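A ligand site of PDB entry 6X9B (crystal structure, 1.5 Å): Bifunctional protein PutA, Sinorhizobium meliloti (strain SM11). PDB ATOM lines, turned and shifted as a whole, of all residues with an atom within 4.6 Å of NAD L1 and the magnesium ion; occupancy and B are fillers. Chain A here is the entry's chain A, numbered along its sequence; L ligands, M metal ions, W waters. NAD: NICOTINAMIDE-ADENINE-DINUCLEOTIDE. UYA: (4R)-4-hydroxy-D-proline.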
ATOM      1  N   ILE A 705      33.080  26.190 -11.521  1.00  0.00           N
ATOM      2  CA  ILE A 705      32.141  25.270 -10.889  1.00  0.00           C
ATOM      3  C   ILE A 705      31.373  24.578 -12.004  1.00  0.00           C
ATOM      4  O   ILE A 705      30.775  25.249 -12.852  1.00  0.00           O
ATOM      5  CB  ILE A 705      31.212  26.015  -9.922  1.00  0.00           C
ATOM      6  CG1 ILE A 705      31.988  26.503  -8.699  1.00  0.00           C
ATOM      7  CG2 ILE A 705      30.045  25.140  -9.497  1.00  0.00           C
ATOM      8  CD1 ILE A 705      31.252  27.530  -7.880  1.00  0.00           C
ATOM      9  N   SER A 706      31.382  23.254 -12.001  1.00  0.00           N
ATOM     10  CA  SER A 706      30.958  22.475 -13.156  1.00  0.00           C
ATOM     11  C   SER A 706      29.923  21.444 -12.758  1.00  0.00           C
ATOM     12  O   SER A 706      29.842  21.049 -11.585  1.00  0.00           O
ATOM     13  CB  SER A 706      32.156  21.776 -13.806  1.00  0.00           C
ATOM     14  OG  SER A 706      32.887  21.014 -12.854  1.00  0.00           O
ATOM     15  N   PRO A 707      29.135  20.956 -13.712  1.00  0.00           N
ATOM     16  CA  PRO A 707      28.085  19.969 -13.413  1.00  0.00           C
ATOM     17  C   PRO A 707      28.581  18.541 -13.610  1.00  0.00           C
ATOM     18  O   PRO A 707      29.644  18.297 -14.168  1.00  0.00           O
ATOM     19  CB  PRO A 707      27.029  20.307 -14.477  1.00  0.00           C
ATOM     20  CG  PRO A 707      27.853  20.730 -15.656  1.00  0.00           C
ATOM     21  CD  PRO A 707      29.026  21.471 -15.090  1.00  0.00           C
ATOM     22  N   TRP A 708      27.784  17.592 -13.130  1.00  0.00           N
ATOM     23  CA  TRP A 708      28.192  16.193 -13.228  1.00  0.00           C
ATOM     24  C   TRP A 708      28.026  15.639 -14.637  1.00  0.00           C
ATOM     25  O   TRP A 708      28.678  14.638 -14.967  1.00  0.00           O
ATOM     26  CB  TRP A 708      27.405  15.309 -12.236  1.00  0.00           C
ATOM     27  CG  TRP A 708      26.023  15.105 -12.706  1.00  0.00           C
ATOM     28  CD1 TRP A 708      24.933  15.827 -12.362  1.00  0.00           C
ATOM     29  CD2 TRP A 708      25.587  14.153 -13.690  1.00  0.00           C
ATOM     30  NE1 TRP A 708      23.835  15.380 -13.041  1.00  0.00           N
ATOM     31  CE2 TRP A 708      24.214  14.354 -13.858  1.00  0.00           C
ATOM     32  CE3 TRP A 708      26.225  13.141 -14.407  1.00  0.00           C
ATOM     33  CZ2 TRP A 708      23.456  13.588 -14.745  1.00  0.00           C
ATOM     34  CZ3 TRP A 708      25.484  12.379 -15.285  1.00  0.00           C
ATOM     35  CH2 TRP A 708      24.114  12.602 -15.447  1.00  0.00           C
ATOM     36  N   ASN A 709      27.205  16.260 -15.483  1.00  0.00           N
ATOM     37  CA  ASN A 709      26.739  15.576 -16.696  1.00  0.00           C
ATOM     38  C   ASN A 709      27.691  15.682 -17.859  1.00  0.00           C
ATOM     39  O   ASN A 709      27.581  14.896 -18.812  1.00  0.00           O
ATOM     40  CB  ASN A 709      25.338  16.056 -17.101  1.00  0.00           C
ATOM     41  CG  ASN A 709      25.321  17.480 -17.577  1.00  0.00           C
ATOM     42  OD1 ASN A 709      25.911  18.367 -16.953  1.00  0.00           O
ATOM     43  ND2 ASN A 709      24.621  17.724 -18.676  1.00  0.00           N
ATOM     44  N   PHE A 710      28.626  16.622 -17.826  1.00  0.00           N
ATOM     45  CA  PHE A 710      29.791  16.631 -18.710  1.00  0.00           C
ATOM     46  C   PHE A 710      31.006  16.787 -17.820  1.00  0.00           C
ATOM     47  O   PHE A 710      31.645  17.842 -17.785  1.00  0.00           O
ATOM     48  CB  PHE A 710      29.686  17.687 -19.805  1.00  0.00           C
ATOM     49  CG  PHE A 710      28.666  17.318 -20.826  1.00  0.00           C
ATOM     50  CD1 PHE A 710      28.988  16.467 -21.861  1.00  0.00           C
ATOM     51  CD2 PHE A 710      27.346  17.728 -20.692  1.00  0.00           C
ATOM     52  CE1 PHE A 710      28.027  16.079 -22.789  1.00  0.00           C
ATOM     53  CE2 PHE A 710      26.385  17.350 -21.606  1.00  0.00           C
ATOM     54  CZ  PHE A 710      26.735  16.519 -22.657  1.00  0.00           C
ATOM     55  N   ILE A 714      32.891  19.959 -19.970  1.00  0.00           N
ATOM     56  CA  ILE A 714      32.586  21.291 -19.458  1.00  0.00           C
ATOM     57  C   ILE A 714      33.541  21.674 -18.329  1.00  0.00           C
ATOM     58  O   ILE A 714      33.965  22.835 -18.219  1.00  0.00           O
ATOM     59  CB  ILE A 714      31.102  21.398 -19.030  1.00  0.00           C
ATOM     60  CG1 ILE A 714      30.195  21.289 -20.255  1.00  0.00           C
ATOM     61  CG2 ILE A 714      30.853  22.665 -18.207  1.00  0.00           C
ATOM     62  CD1 ILE A 714      28.726  21.153 -19.920  1.00  0.00           C
ATOM     63  N   LYS A 732      36.156  23.367  -8.969  1.00  0.00           N
ATOM     64  CA  LYS A 732      35.225  22.694  -8.059  1.00  0.00           C
ATOM     65  C   LYS A 732      34.310  21.812  -8.904  1.00  0.00           C
ATOM     66  O   LYS A 732      33.293  22.296  -9.422  1.00  0.00           O
ATOM     67  CB  LYS A 732      34.446  23.706  -7.219  1.00  0.00           C
ATOM     68  CG  LYS A 732      34.131  23.273  -5.784  1.00  0.00           C
ATOM     69  CD  LYS A 732      33.306  21.994  -5.735  1.00  0.00           C
ATOM     70  CE  LYS A 732      31.874  22.217  -6.226  1.00  0.00           C
ATOM     71  NZ  LYS A 732      31.143  20.898  -6.218  1.00  0.00           N
ATOM     72  N   PRO A 733      34.638  20.539  -9.071  1.00  0.00           N
ATOM     73  CA  PRO A 733      33.779  19.650  -9.865  1.00  0.00           C
ATOM     74  C   PRO A 733      32.547  19.246  -9.082  1.00  0.00           C
ATOM     75  O   PRO A 733      32.502  19.334  -7.861  1.00  0.00           O
ATOM     76  CB  PRO A 733      34.673  18.436 -10.098  1.00  0.00           C
ATOM     77  CG  PRO A 733      35.545  18.378  -8.893  1.00  0.00           C
ATOM     78  CD  PRO A 733      35.792  19.821  -8.489  1.00  0.00           C
ATOM     79  N   ALA A 734      31.531  18.798  -9.822  1.00  0.00           N
ATOM     80  CA  ALA A 734      30.318  18.295  -9.188  1.00  0.00           C
ATOM     81  C   ALA A 734      30.672  17.179  -8.209  1.00  0.00           C
ATOM     82  O   ALA A 734      31.621  16.423  -8.414  1.00  0.00           O
ATOM     83  CB  ALA A 734      29.339  17.773 -10.246  1.00  0.00           C
ATOM     84  N   GLU A 735      29.919  17.088  -7.113  1.00  0.00           N
ATOM     85  CA  GLU A 735      30.222  16.071  -6.115  1.00  0.00           C
ATOM     86  C   GLU A 735      30.042  14.659  -6.673  1.00  0.00           C
ATOM     87  O   GLU A 735      30.705  13.727  -6.205  1.00  0.00           O
ATOM     88  CB  GLU A 735      29.373  16.276  -4.852  1.00  0.00           C
ATOM     89  CG  GLU A 735      27.877  16.325  -5.082  1.00  0.00           C
ATOM     90  CD  GLU A 735      27.380  17.733  -5.416  1.00  0.00           C
ATOM     91  OE1 GLU A 735      28.151  18.504  -6.030  1.00  0.00           O
ATOM     92  OE2 GLU A 735      26.239  18.070  -5.060  1.00  0.00           O
ATOM     93  N   GLY A 763      34.169  18.283  -3.724  1.00  0.00           N
ATOM     94  CA  GLY A 763      33.170  18.412  -2.680  1.00  0.00           C
ATOM     95  C   GLY A 763      31.861  18.920  -3.239  1.00  0.00           C
ATOM     96  O   GLY A 763      31.695  19.049  -4.448  1.00  0.00           O
ATOM     97  N   ASP A 764      30.946  19.211  -2.321  1.00  0.00           N
ATOM     98  CA  ASP A 764      29.569  19.537  -2.669  1.00  0.00           C
ATOM     99  C   ASP A 764      29.378  21.044  -2.838  1.00  0.00           C
ATOM    100  O   ASP A 764      30.347  21.805  -2.965  1.00  0.00           O
ATOM    101  CB  ASP A 764      28.595  18.888  -1.674  1.00  0.00           C
ATOM    102  CG  ASP A 764      28.806  19.371  -0.246  1.00  0.00           C
ATOM    103  OD1 ASP A 764      29.374  20.466  -0.044  1.00  0.00           O
ATOM    104  OD2 ASP A 764      28.395  18.644   0.673  1.00  0.00           O
ATOM    105  N   GLY A 765      28.128  21.515  -2.837  1.00  0.00           N
ATOM    106  CA  GLY A 765      27.852  22.924  -3.059  1.00  0.00           C
ATOM    107  C   GLY A 765      28.386  23.838  -1.977  1.00  0.00           C
ATOM    108  O   GLY A 765      28.535  25.037  -2.215  1.00  0.00           O
ATOM    109  N   GLY A 768      31.679  24.842  -3.287  1.00  0.00           N
ATOM    110  CA  GLY A 768      31.457  25.846  -4.316  1.00  0.00           C
ATOM    111  C   GLY A 768      31.142  27.201  -3.712  1.00  0.00           C
ATOM    112  O   GLY A 768      31.696  28.226  -4.138  1.00  0.00           O
ATOM    113  N   ALA A 769      30.271  27.226  -2.718  1.00  0.00           N
ATOM    114  CA  ALA A 769      29.856  28.497  -2.127  1.00  0.00           C
ATOM    115  C   ALA A 769      31.002  29.154  -1.365  1.00  0.00           C
ATOM    116  O   ALA A 769      31.163  30.375  -1.386  1.00  0.00           O
ATOM    117  CB  ALA A 769      28.635  28.280  -1.227  1.00  0.00           C
ATOM    118  N   PHE A 782      30.319  29.226 -14.003  1.00  0.00           N
ATOM    119  CA  PHE A 782      29.377  28.269 -13.472  1.00  0.00           C
ATOM    120  C   PHE A 782      28.590  27.657 -14.614  1.00  0.00           C
ATOM    121  O   PHE A 782      28.009  28.374 -15.431  1.00  0.00           O
ATOM    122  CB  PHE A 782      28.387  28.954 -12.515  1.00  0.00           C
ATOM    123  CG  PHE A 782      27.287  28.045 -12.064  1.00  0.00           C
ATOM    124  CD1 PHE A 782      27.495  27.173 -11.013  1.00  0.00           C
ATOM    125  CD2 PHE A 782      26.044  28.074 -12.686  1.00  0.00           C
ATOM    126  CE1 PHE A 782      26.484  26.326 -10.584  1.00  0.00           C
ATOM    127  CE2 PHE A 782      25.025  27.225 -12.261  1.00  0.00           C
ATOM    128  CZ  PHE A 782      25.252  26.348 -11.201  1.00  0.00           C
ATOM    129  N   THR A 783      28.562  26.335 -14.652  1.00  0.00           N
ATOM    130  CA  THR A 783      27.599  25.614 -15.472  1.00  0.00           C
ATOM    131  C   THR A 783      26.834  24.668 -14.552  1.00  0.00           C
ATOM    132  O   THR A 783      27.448  23.952 -13.751  1.00  0.00           O
ATOM    133  CB  THR A 783      28.311  24.894 -16.612  1.00  0.00           C
ATOM    134  OG1 THR A 783      29.079  25.851 -17.357  1.00  0.00           O
ATOM    135  CG2 THR A 783      27.304  24.249 -17.518  1.00  0.00           C
ATOM    136  N   GLY A 784      25.511  24.731 -14.612  1.00  0.00           N
ATOM    137  CA  GLY A 784      24.679  23.994 -13.678  1.00  0.00           C
ATOM    138  C   GLY A 784      23.240  24.493 -13.733  1.00  0.00           C
ATOM    139  O   GLY A 784      22.827  25.117 -14.715  1.00  0.00           O
ATOM    140  N   SER A 785      22.489  24.196 -12.682  1.00  0.00           N
ATOM    141  CA  SER A 785      21.071  24.558 -12.643  1.00  0.00           C
ATOM    142  C   SER A 785      20.889  26.069 -12.498  1.00  0.00           C
ATOM    143  O   SER A 785      21.715  26.760 -11.901  1.00  0.00           O
ATOM    144  CB  SER A 785      20.367  23.849 -11.490  1.00  0.00           C
ATOM    145  OG  SER A 785      20.818  24.325 -10.229  1.00  0.00           O
ATOM    146  N   VAL A 788      20.796  27.222  -8.730  1.00  0.00           N
ATOM    147  CA  VAL A 788      22.092  27.408  -8.079  1.00  0.00           C
ATOM    148  C   VAL A 788      22.783  28.654  -8.626  1.00  0.00           C
ATOM    149  O   VAL A 788      23.372  29.437  -7.866  1.00  0.00           O
ATOM    150  CB  VAL A 788      22.951  26.147  -8.226  1.00  0.00           C
ATOM    151  CG1 VAL A 788      24.374  26.428  -7.764  1.00  0.00           C
ATOM    152  CG2 VAL A 788      22.370  25.035  -7.399  1.00  0.00           C
ATOM    153  N   LEU A 791      21.653  31.633  -6.720  1.00  0.00           N
ATOM    154  CA  LEU A 791      22.309  31.783  -5.428  1.00  0.00           C
ATOM    155  C   LEU A 791      23.700  32.377  -5.586  1.00  0.00           C
ATOM    156  O   LEU A 791      24.103  33.235  -4.789  1.00  0.00           O
ATOM    157  CB  LEU A 791      22.365  30.440  -4.708  1.00  0.00           C
ATOM    158  CG  LEU A 791      21.022  29.934  -4.199  1.00  0.00           C
ATOM    159  CD1 LEU A 791      21.151  28.474  -3.902  1.00  0.00           C
ATOM    160  CD2 LEU A 791      20.589  30.706  -2.952  1.00  0.00           C
ATOM    161  N   ILE A 792      24.435  31.941  -6.616  1.00  0.00           N
ATOM    162  CA  ILE A 792      25.766  32.510  -6.844  1.00  0.00           C
ATOM    163  C   ILE A 792      25.659  33.983  -7.228  1.00  0.00           C
ATOM    164  O   ILE A 792      26.385  34.836  -6.703  1.00  0.00           O
ATOM    165  CB  ILE A 792      26.531  31.686  -7.900  1.00  0.00           C
ATOM    166  CG1 ILE A 792      26.879  30.331  -7.332  1.00  0.00           C
ATOM    167  CG2 ILE A 792      27.815  32.431  -8.340  1.00  0.00           C
ATOM    168  CD1 ILE A 792      27.383  29.370  -8.380  1.00  0.00           C
ATOM    169  N   GLU A 812      25.875  29.374 -17.141  1.00  0.00           N
ATOM    170  CA  GLU A 812      25.273  28.661 -18.246  1.00  0.00           C
ATOM    171  C   GLU A 812      24.367  27.585 -17.655  1.00  0.00           C
ATOM    172  O   GLU A 812      24.850  26.686 -16.951  1.00  0.00           O
ATOM    173  CB  GLU A 812      26.364  28.079 -19.140  1.00  0.00           C
ATOM    174  CG  GLU A 812      27.278  29.178 -19.734  1.00  0.00           C
ATOM    175  CD  GLU A 812      26.481  30.204 -20.534  1.00  0.00           C
ATOM    176  OE1 GLU A 812      26.163  29.934 -21.715  1.00  0.00           O
ATOM    177  OE2 GLU A 812      26.133  31.267 -19.979  1.00  0.00           O
ATOM    178  N   THR A 813      23.073  27.711 -17.904  1.00  0.00           N
ATOM    179  CA  THR A 813      22.092  27.028 -17.068  1.00  0.00           C
ATOM    180  C   THR A 813      21.141  26.119 -17.856  1.00  0.00           C
ATOM    181  O   THR A 813      21.485  25.645 -18.932  1.00  0.00           O
ATOM    182  CB  THR A 813      21.395  28.051 -16.149  1.00  0.00           C
ATOM    183  OG1 THR A 813      20.906  29.153 -16.925  1.00  0.00           O
ATOM    184  CG2 THR A 813      22.381  28.586 -15.108  1.00  0.00           C
ATOM    185  N   GLY A 814      19.941  25.879 -17.316  1.00  0.00           N
ATOM    186  CA  GLY A 814      19.101  24.810 -17.845  1.00  0.00           C
ATOM    187  C   GLY A 814      18.351  25.186 -19.111  1.00  0.00           C
ATOM    188  O   GLY A 814      18.351  26.320 -19.575  1.00  0.00           O
ATOM    189  N   GLY A 815      17.666  24.180 -19.672  1.00  0.00           N
ATOM    190  CA  GLY A 815      16.875  24.380 -20.861  1.00  0.00           C
ATOM    191  C   GLY A 815      15.507  23.733 -20.738  1.00  0.00           C
ATOM    192  O   GLY A 815      15.272  22.888 -19.882  1.00  0.00           O
ATOM    193  N   CYS A 846      22.138  19.024 -21.066  1.00  0.00           N
ATOM    194  CA  CYS A 846      21.397  20.274 -20.976  1.00  0.00           C
ATOM    195  C   CYS A 846      20.721  20.604 -22.306  1.00  0.00           C
ATOM    196  O   CYS A 846      19.674  21.267 -22.320  1.00  0.00           O
ATOM    197  CB  CYS A 846      22.305  21.423 -20.544  1.00  0.00           C
ATOM    198  SG  CYS A 846      23.791  21.572 -21.519  1.00  0.00           S
ATOM    199  N   GLU A 942      12.648  22.400 -15.843  1.00  0.00           N
ATOM    200  CA  GLU A 942      13.426  21.389 -16.535  1.00  0.00           C
ATOM    201  C   GLU A 942      13.404  20.090 -15.742  1.00  0.00           C
ATOM    202  O   GLU A 942      13.691  20.085 -14.535  1.00  0.00           O
ATOM    203  CB  GLU A 942      14.869  21.903 -16.661  1.00  0.00           C
ATOM    204  CG  GLU A 942      15.874  20.914 -17.222  1.00  0.00           C
ATOM    205  CD  GLU A 942      17.319  21.400 -17.068  1.00  0.00           C
ATOM    206  OE1 GLU A 942      18.022  21.522 -18.091  1.00  0.00           O
ATOM    207  OE2 GLU A 942      17.736  21.672 -15.916  1.00  0.00           O
ATOM    208  N   PHE A 944      15.285  16.814 -15.610  1.00  0.00           N
ATOM    209  CA  PHE A 944      16.592  16.437 -16.155  1.00  0.00           C
ATOM    210  C   PHE A 944      16.714  14.920 -16.172  1.00  0.00           C
ATOM    211  O   PHE A 944      17.383  14.294 -15.346  1.00  0.00           O
ATOM    212  CB  PHE A 944      17.709  17.071 -15.333  1.00  0.00           C
ATOM    213  CG  PHE A 944      18.962  17.290 -16.102  1.00  0.00           C
ATOM    214  CD1 PHE A 944      19.006  18.212 -17.140  1.00  0.00           C
ATOM    215  CD2 PHE A 944      20.130  16.593 -15.783  1.00  0.00           C
ATOM    216  CE1 PHE A 944      20.150  18.414 -17.854  1.00  0.00           C
ATOM    217  CE2 PHE A 944      21.296  16.813 -16.504  1.00  0.00           C
ATOM    218  CZ  PHE A 944      21.299  17.733 -17.553  1.00  0.00           C
ATOM    219  N   LEU A 972      17.763  27.585 -24.776  1.00  0.00           N
ATOM    220  CA  LEU A 972      19.041  26.911 -24.933  1.00  0.00           C
ATOM    221  C   LEU A 972      19.146  26.286 -26.324  1.00  0.00           C
ATOM    222  O   LEU A 972      19.691  26.918 -27.243  1.00  0.00           O
ATOM    223  CB  LEU A 972      19.268  25.923 -23.795  1.00  0.00           C
ATOM    224  CG  LEU A 972      20.629  25.242 -23.741  1.00  0.00           C
ATOM    225  CD1 LEU A 972      21.735  26.275 -23.807  1.00  0.00           C
ATOM    226  CD2 LEU A 972      20.728  24.486 -22.433  1.00  0.00           C
ATOM    227  N   PHE A1012      28.259  27.003 -28.129  1.00  0.00           N
ATOM    228  CA  PHE A1012      27.128  26.517 -27.358  1.00  0.00           C
ATOM    229  C   PHE A1012      26.786  27.460 -26.210  1.00  0.00           C
ATOM    230  O   PHE A1012      27.663  27.883 -25.443  1.00  0.00           O
ATOM    231  CB  PHE A1012      27.363  25.098 -26.851  1.00  0.00           C
ATOM    232  CG  PHE A1012      26.173  24.514 -26.155  1.00  0.00           C
ATOM    233  CD1 PHE A1012      25.116  23.989 -26.888  1.00  0.00           C
ATOM    234  CD2 PHE A1012      26.099  24.497 -24.768  1.00  0.00           C
ATOM    235  CE1 PHE A1012      24.016  23.469 -26.258  1.00  0.00           C
ATOM    236  CE2 PHE A1012      24.995  23.976 -24.129  1.00  0.00           C
ATOM    237  CZ  PHE A1012      23.945  23.443 -24.871  1.00  0.00           C
ATOM    238  N   SER A1018      18.463  30.236 -19.527  1.00  0.00           N
ATOM    239  CA  SER A1018      19.449  29.242 -19.927  1.00  0.00           C
ATOM    240  C   SER A1018      20.884  29.767 -19.941  1.00  0.00           C
ATOM    241  O   SER A1018      21.799  28.968 -20.127  1.00  0.00           O
ATOM    242  CB  SER A1018      19.131  28.723 -21.336  1.00  0.00           C
ATOM    243  OG  SER A1018      17.848  28.154 -21.359  1.00  0.00           O
HETATM  244  PA  NAD L   1      23.802  21.818 -10.007  1.00  0.00           P
HETATM  245  O1A NAD L   1      23.190  23.181 -10.031  1.00  0.00           O
HETATM  246  O2A NAD L   1      23.044  20.896  -9.089  1.00  0.00           O
HETATM  247  O5B NAD L   1      25.392  21.795  -9.539  1.00  0.00           O
HETATM  248  C5B NAD L   1      26.393  22.288 -10.420  1.00  0.00           C
HETATM  249  C4B NAD L   1      27.643  22.634  -9.539  1.00  0.00           C
HETATM  250  O4B NAD L   1      27.212  23.776  -8.482  1.00  0.00           O
HETATM  251  C3B NAD L   1      28.076  21.613  -8.830  1.00  0.00           C
HETATM  252  O3B NAD L   1      29.579  21.613  -8.847  1.00  0.00           O
HETATM  253  C2B NAD L   1      27.552  21.848  -7.384  1.00  0.00           C
HETATM  254  O2B NAD L   1      28.325  21.206  -6.442  1.00  0.00           O
HETATM  255  C1B NAD L   1      27.612  23.387  -7.282  1.00  0.00           C
HETATM  256  N9A NAD L   1      26.696  23.923  -6.275  1.00  0.00           N
HETATM  257  C8A NAD L   1      25.555  23.551  -5.690  1.00  0.00           C
HETATM  258  N7A NAD L   1      25.201  24.542  -4.857  1.00  0.00           N
HETATM  259  C5A NAD L   1      26.121  25.526  -4.924  1.00  0.00           C
HETATM  260  C6A NAD L   1      26.209  26.755  -4.260  1.00  0.00           C
HETATM  261  N6A NAD L   1      25.168  27.158  -3.278  1.00  0.00           N
HETATM  262  N1A NAD L   1      27.219  27.568  -4.503  1.00  0.00           N
HETATM  263  C2A NAD L   1      28.193  27.192  -5.422  1.00  0.00           C
HETATM  264  N3A NAD L   1      28.120  25.999  -6.070  1.00  0.00           N
HETATM  265  C4A NAD L   1      27.054  25.157  -5.816  1.00  0.00           C
HETATM  266  O3  NAD L   1      23.790  21.269 -11.542  1.00  0.00           O
HETATM  267  PN  NAD L   1      24.111  19.686 -11.999  1.00  0.00           P
HETATM  268  O1N NAD L   1      23.016  18.809 -11.345  1.00  0.00           O
HETATM  269  O2N NAD L   1      25.497  19.255 -11.614  1.00  0.00           O
HETATM  270  O5D NAD L   1      23.929  19.667 -13.627  1.00  0.00           O
HETATM  271  C5D NAD L   1      22.619  19.650 -14.190  1.00  0.00           C
HETATM  272  C4D NAD L   1      22.126  21.050 -14.547  1.00  0.00           C
HETATM  273  O4D NAD L   1      23.287  21.810 -15.343  1.00  0.00           O
HETATM  274  C3D NAD L   1      21.071  21.015 -15.362  1.00  0.00           C
HETATM  275  O3D NAD L   1      20.052  22.059 -14.910  1.00  0.00           O
HETATM  276  C2D NAD L   1      21.599  21.313 -16.731  1.00  0.00           C
HETATM  277  O2D NAD L   1      20.662  21.847 -17.621  1.00  0.00           O
HETATM  278  C1D NAD L   1      22.712  22.341 -16.348  1.00  0.00           C
HETATM  279  N1N NAD L   1      23.689  22.378 -17.457  1.00  0.00           N
HETATM  280  C2N NAD L   1      23.751  23.481 -18.286  1.00  0.00           C
HETATM  281  C3N NAD L   1      24.670  23.442 -19.316  1.00  0.00           C
HETATM  282  C7N NAD L   1      24.804  24.661 -20.288  1.00  0.00           C
HETATM  283  O7N NAD L   1      25.748  24.696 -21.026  1.00  0.00           O
HETATM  284  N7N NAD L   1      23.763  25.715 -20.279  1.00  0.00           N
HETATM  285  C4N NAD L   1      25.513  22.364 -19.465  1.00  0.00           C
HETATM  286  C5N NAD L   1      25.400  21.247 -18.665  1.00  0.00           C
HETATM  287  C6N NAD L   1      24.473  21.284 -17.640  1.00  0.00           C
HETATM  288  N   UYA L   2      28.086  18.966 -24.714  1.00  0.00           N
HETATM  289  CA  UYA L   2      27.404  19.671 -25.848  1.00  0.00           C
HETATM  290  C   UYA L   2      25.971  19.104 -26.003  1.00  0.00           C
HETATM  291  OXT UYA L   2      25.671  18.102 -25.329  1.00  0.00           O
HETATM  292  CB  UYA L   2      27.358  21.170 -25.499  1.00  0.00           C
HETATM  293  CG  UYA L   2      27.356  21.146 -23.963  1.00  0.00           C
HETATM  294  CD  UYA L   2      28.265  19.944 -23.625  1.00  0.00           C
HETATM  295  OD1 UYA L   2      26.071  20.946 -23.502  1.00  0.00           O
HETATM  296  O   UYA L   2      25.223  19.725 -26.812  1.00  0.00           O
HETATM  297 MG    MG M   1      21.799  19.376  -9.180  1.00  0.00          MG
HETATM  298  O   HOH W   1      18.299  24.514 -14.728  1.00  0.00           O
HETATM  299  O   HOH W   2      28.097  25.780 -21.903  1.00  0.00           O
HETATM  300  O   HOH W   3      19.145  20.321 -12.675  1.00  0.00           O
HETATM  301  O   HOH W   4      20.380  20.243 -10.308  1.00  0.00           O
HETATM  302  O   HOH W   5      25.083  30.178  -1.874  1.00  0.00           O
HETATM  303  O   HOH W   6      23.304  19.073  -7.882  1.00  0.00           O
HETATM  304  O   HOH W   7      26.299  18.532  -8.914  1.00  0.00           O
HETATM  305  O   HOH W   8      23.880  28.392 -21.743  1.00  0.00           O
HETATM  306  O   HOH W   9      27.048  30.318  -3.604  1.00  0.00           O
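N of Trp 708 lies within hydrogen-bond range of O2N of NAD L1 (3.2 Å).
O1A of NAD L1 sits at hydrogen-bond distance from OG of Ser 785 (2.6 Å).
The backbone carbonyl oxygen of Thr 813 lies within hydrogen-bond range of a nitrogen (N7N) of NAD L1 (2.6 Å).
An oxygen (O7N) of NAD L1 sits close to the side-chain sulfur of Cys 846 (3.7 Å).
The side-chain carboxylate (OE1) of Glu 735 sits at hydrogen-bond distance from an oxygen (O2B) of NAD L1, 2.7 Å away.
An oxygen (O3B) of NAD L1 is in hydrogen-bond range of the backbone carbonyl oxygen of Ser 706.
NZ of Lys 732 lies within hydrogen-bond range of O2B of NAD L1 (2.8 Å).
The side-chain carboxylate of Glu 942 is in hydrogen-bond range of an oxygen (O3D) of NAD L1.
The side-chain sulfur (SG) of Cys 846 sits at hydrogen-bond distance from an oxygen (OD1) of UYA L2.
O1A of NAD L1 sits at hydrogen-bond distance from N of Ser 785, 2.9 Å away.
The side-chain carboxylate (OE1) of Glu 735 is in salt-bridge range of the side-chain amino group (NZ) of Lys 732 (3.8 Å).
O of Gly 763 lies within hydrogen-bond range of NZ of Lys 732 (2.6 Å).
O of Glu 812 is in hydrogen-bond range of N of Gly 784, 3.1 Å away.
The backbone carbonyl oxygen (O) of Asp 764 lies within hydrogen-bond range of the side-chain amino group (NZ) of Lys 732.
The side-chain hydroxyl (OG) of Ser 1018 is in hydrogen-bond range of the backbone NH (N) of Leu 972 (3.5 Å).
The backbone NH of Gly 815 is in hydrogen-bond range of the side-chain carboxylate of Glu 942, 3.1 Å away.
O of Gly 814 lies within hydrogen-bond range of OG of Ser 1018 (2.6 Å).
The backbone NH of Ala 734 lies within hydrogen-bond range of the backbone carbonyl oxygen of Ser 706 (3.3 Å).
An oxygen (O4D) of NAD L1 lies close to the backbone carbonyl oxygen of Gly 784 (3.4 Å).
Merely in contact with NAD L1: Ile 705 (3.3 Å), Pro 707 (3.2 Å), Asn 709 (3.3 Å), Ile 714 (3.5 Å), Pro 733 (3.8 Å), Ala 734 (3.4 Å), Asp 764 (3.8 Å), Gly 765 (3.5 Å), Gly 768 (3.4 Å), Ala 769 (3.4 Å), Phe 782 (3.4 Å), Thr 783 (3.2 Å), Val 788 (3.3 Å), Ile 792 (3.8 Å), Glu 812 (3.3 Å), Gly 814 (3.4 Å), Phe 944 (3.4 Å), Leu 972 (3.9 Å), Phe 1012 (3.3 Å) and Ser 1018 (3.8 Å).
Hydrophobic or aromatic side chains that line NAD L1: Ile 705, Pro 707, Trp 708, Ile 714, Ala 769, Phe 782, Val 788, Ile 792, Phe 944, Leu 972 and Phe 1012.
Within 4 Å of NAD L1: Ile 705, Ser 706, Pro 707, Trp 708, Asn 709, Ile 714, Lys 732, Pro 733, Ala 734, Glu 735, Asp 764, Gly 765, Gly 768, Ala 769, Phe 782, Thr 783, Gly 784, Ser 785, Val 788, Ile 792, Glu 812, Thr 813, Gly 814, Cys 846, Glu 942, Phe 944, Leu 972, Phe 1012 and Ser 1018.
No residue comes within 4 Å of the magnesium ion.
The magnesium ion is bound by an oxygen (O2A) of NAD L1 (2.0 Å), water W4 (2.0 Å), water W6 (2.0 Å) and an oxygen (O1N) of NAD L1 (2.5 Å).
Water W7 lies within hydrogen-bond range of O2N of NAD L1 (2.9 Å) and OE1 of Glu 735 (3.4 Å).
Water W1 lies within hydrogen-bond range of O3D of NAD L1, OE2 of Glu 942 and N of Gly 814.
Water W8 lies within hydrogen-bond range of O of Ser 1018 (2.7 Å), OE1 of Glu 812 (2.8 Å) and N7N of NAD L1 (3.1 Å).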
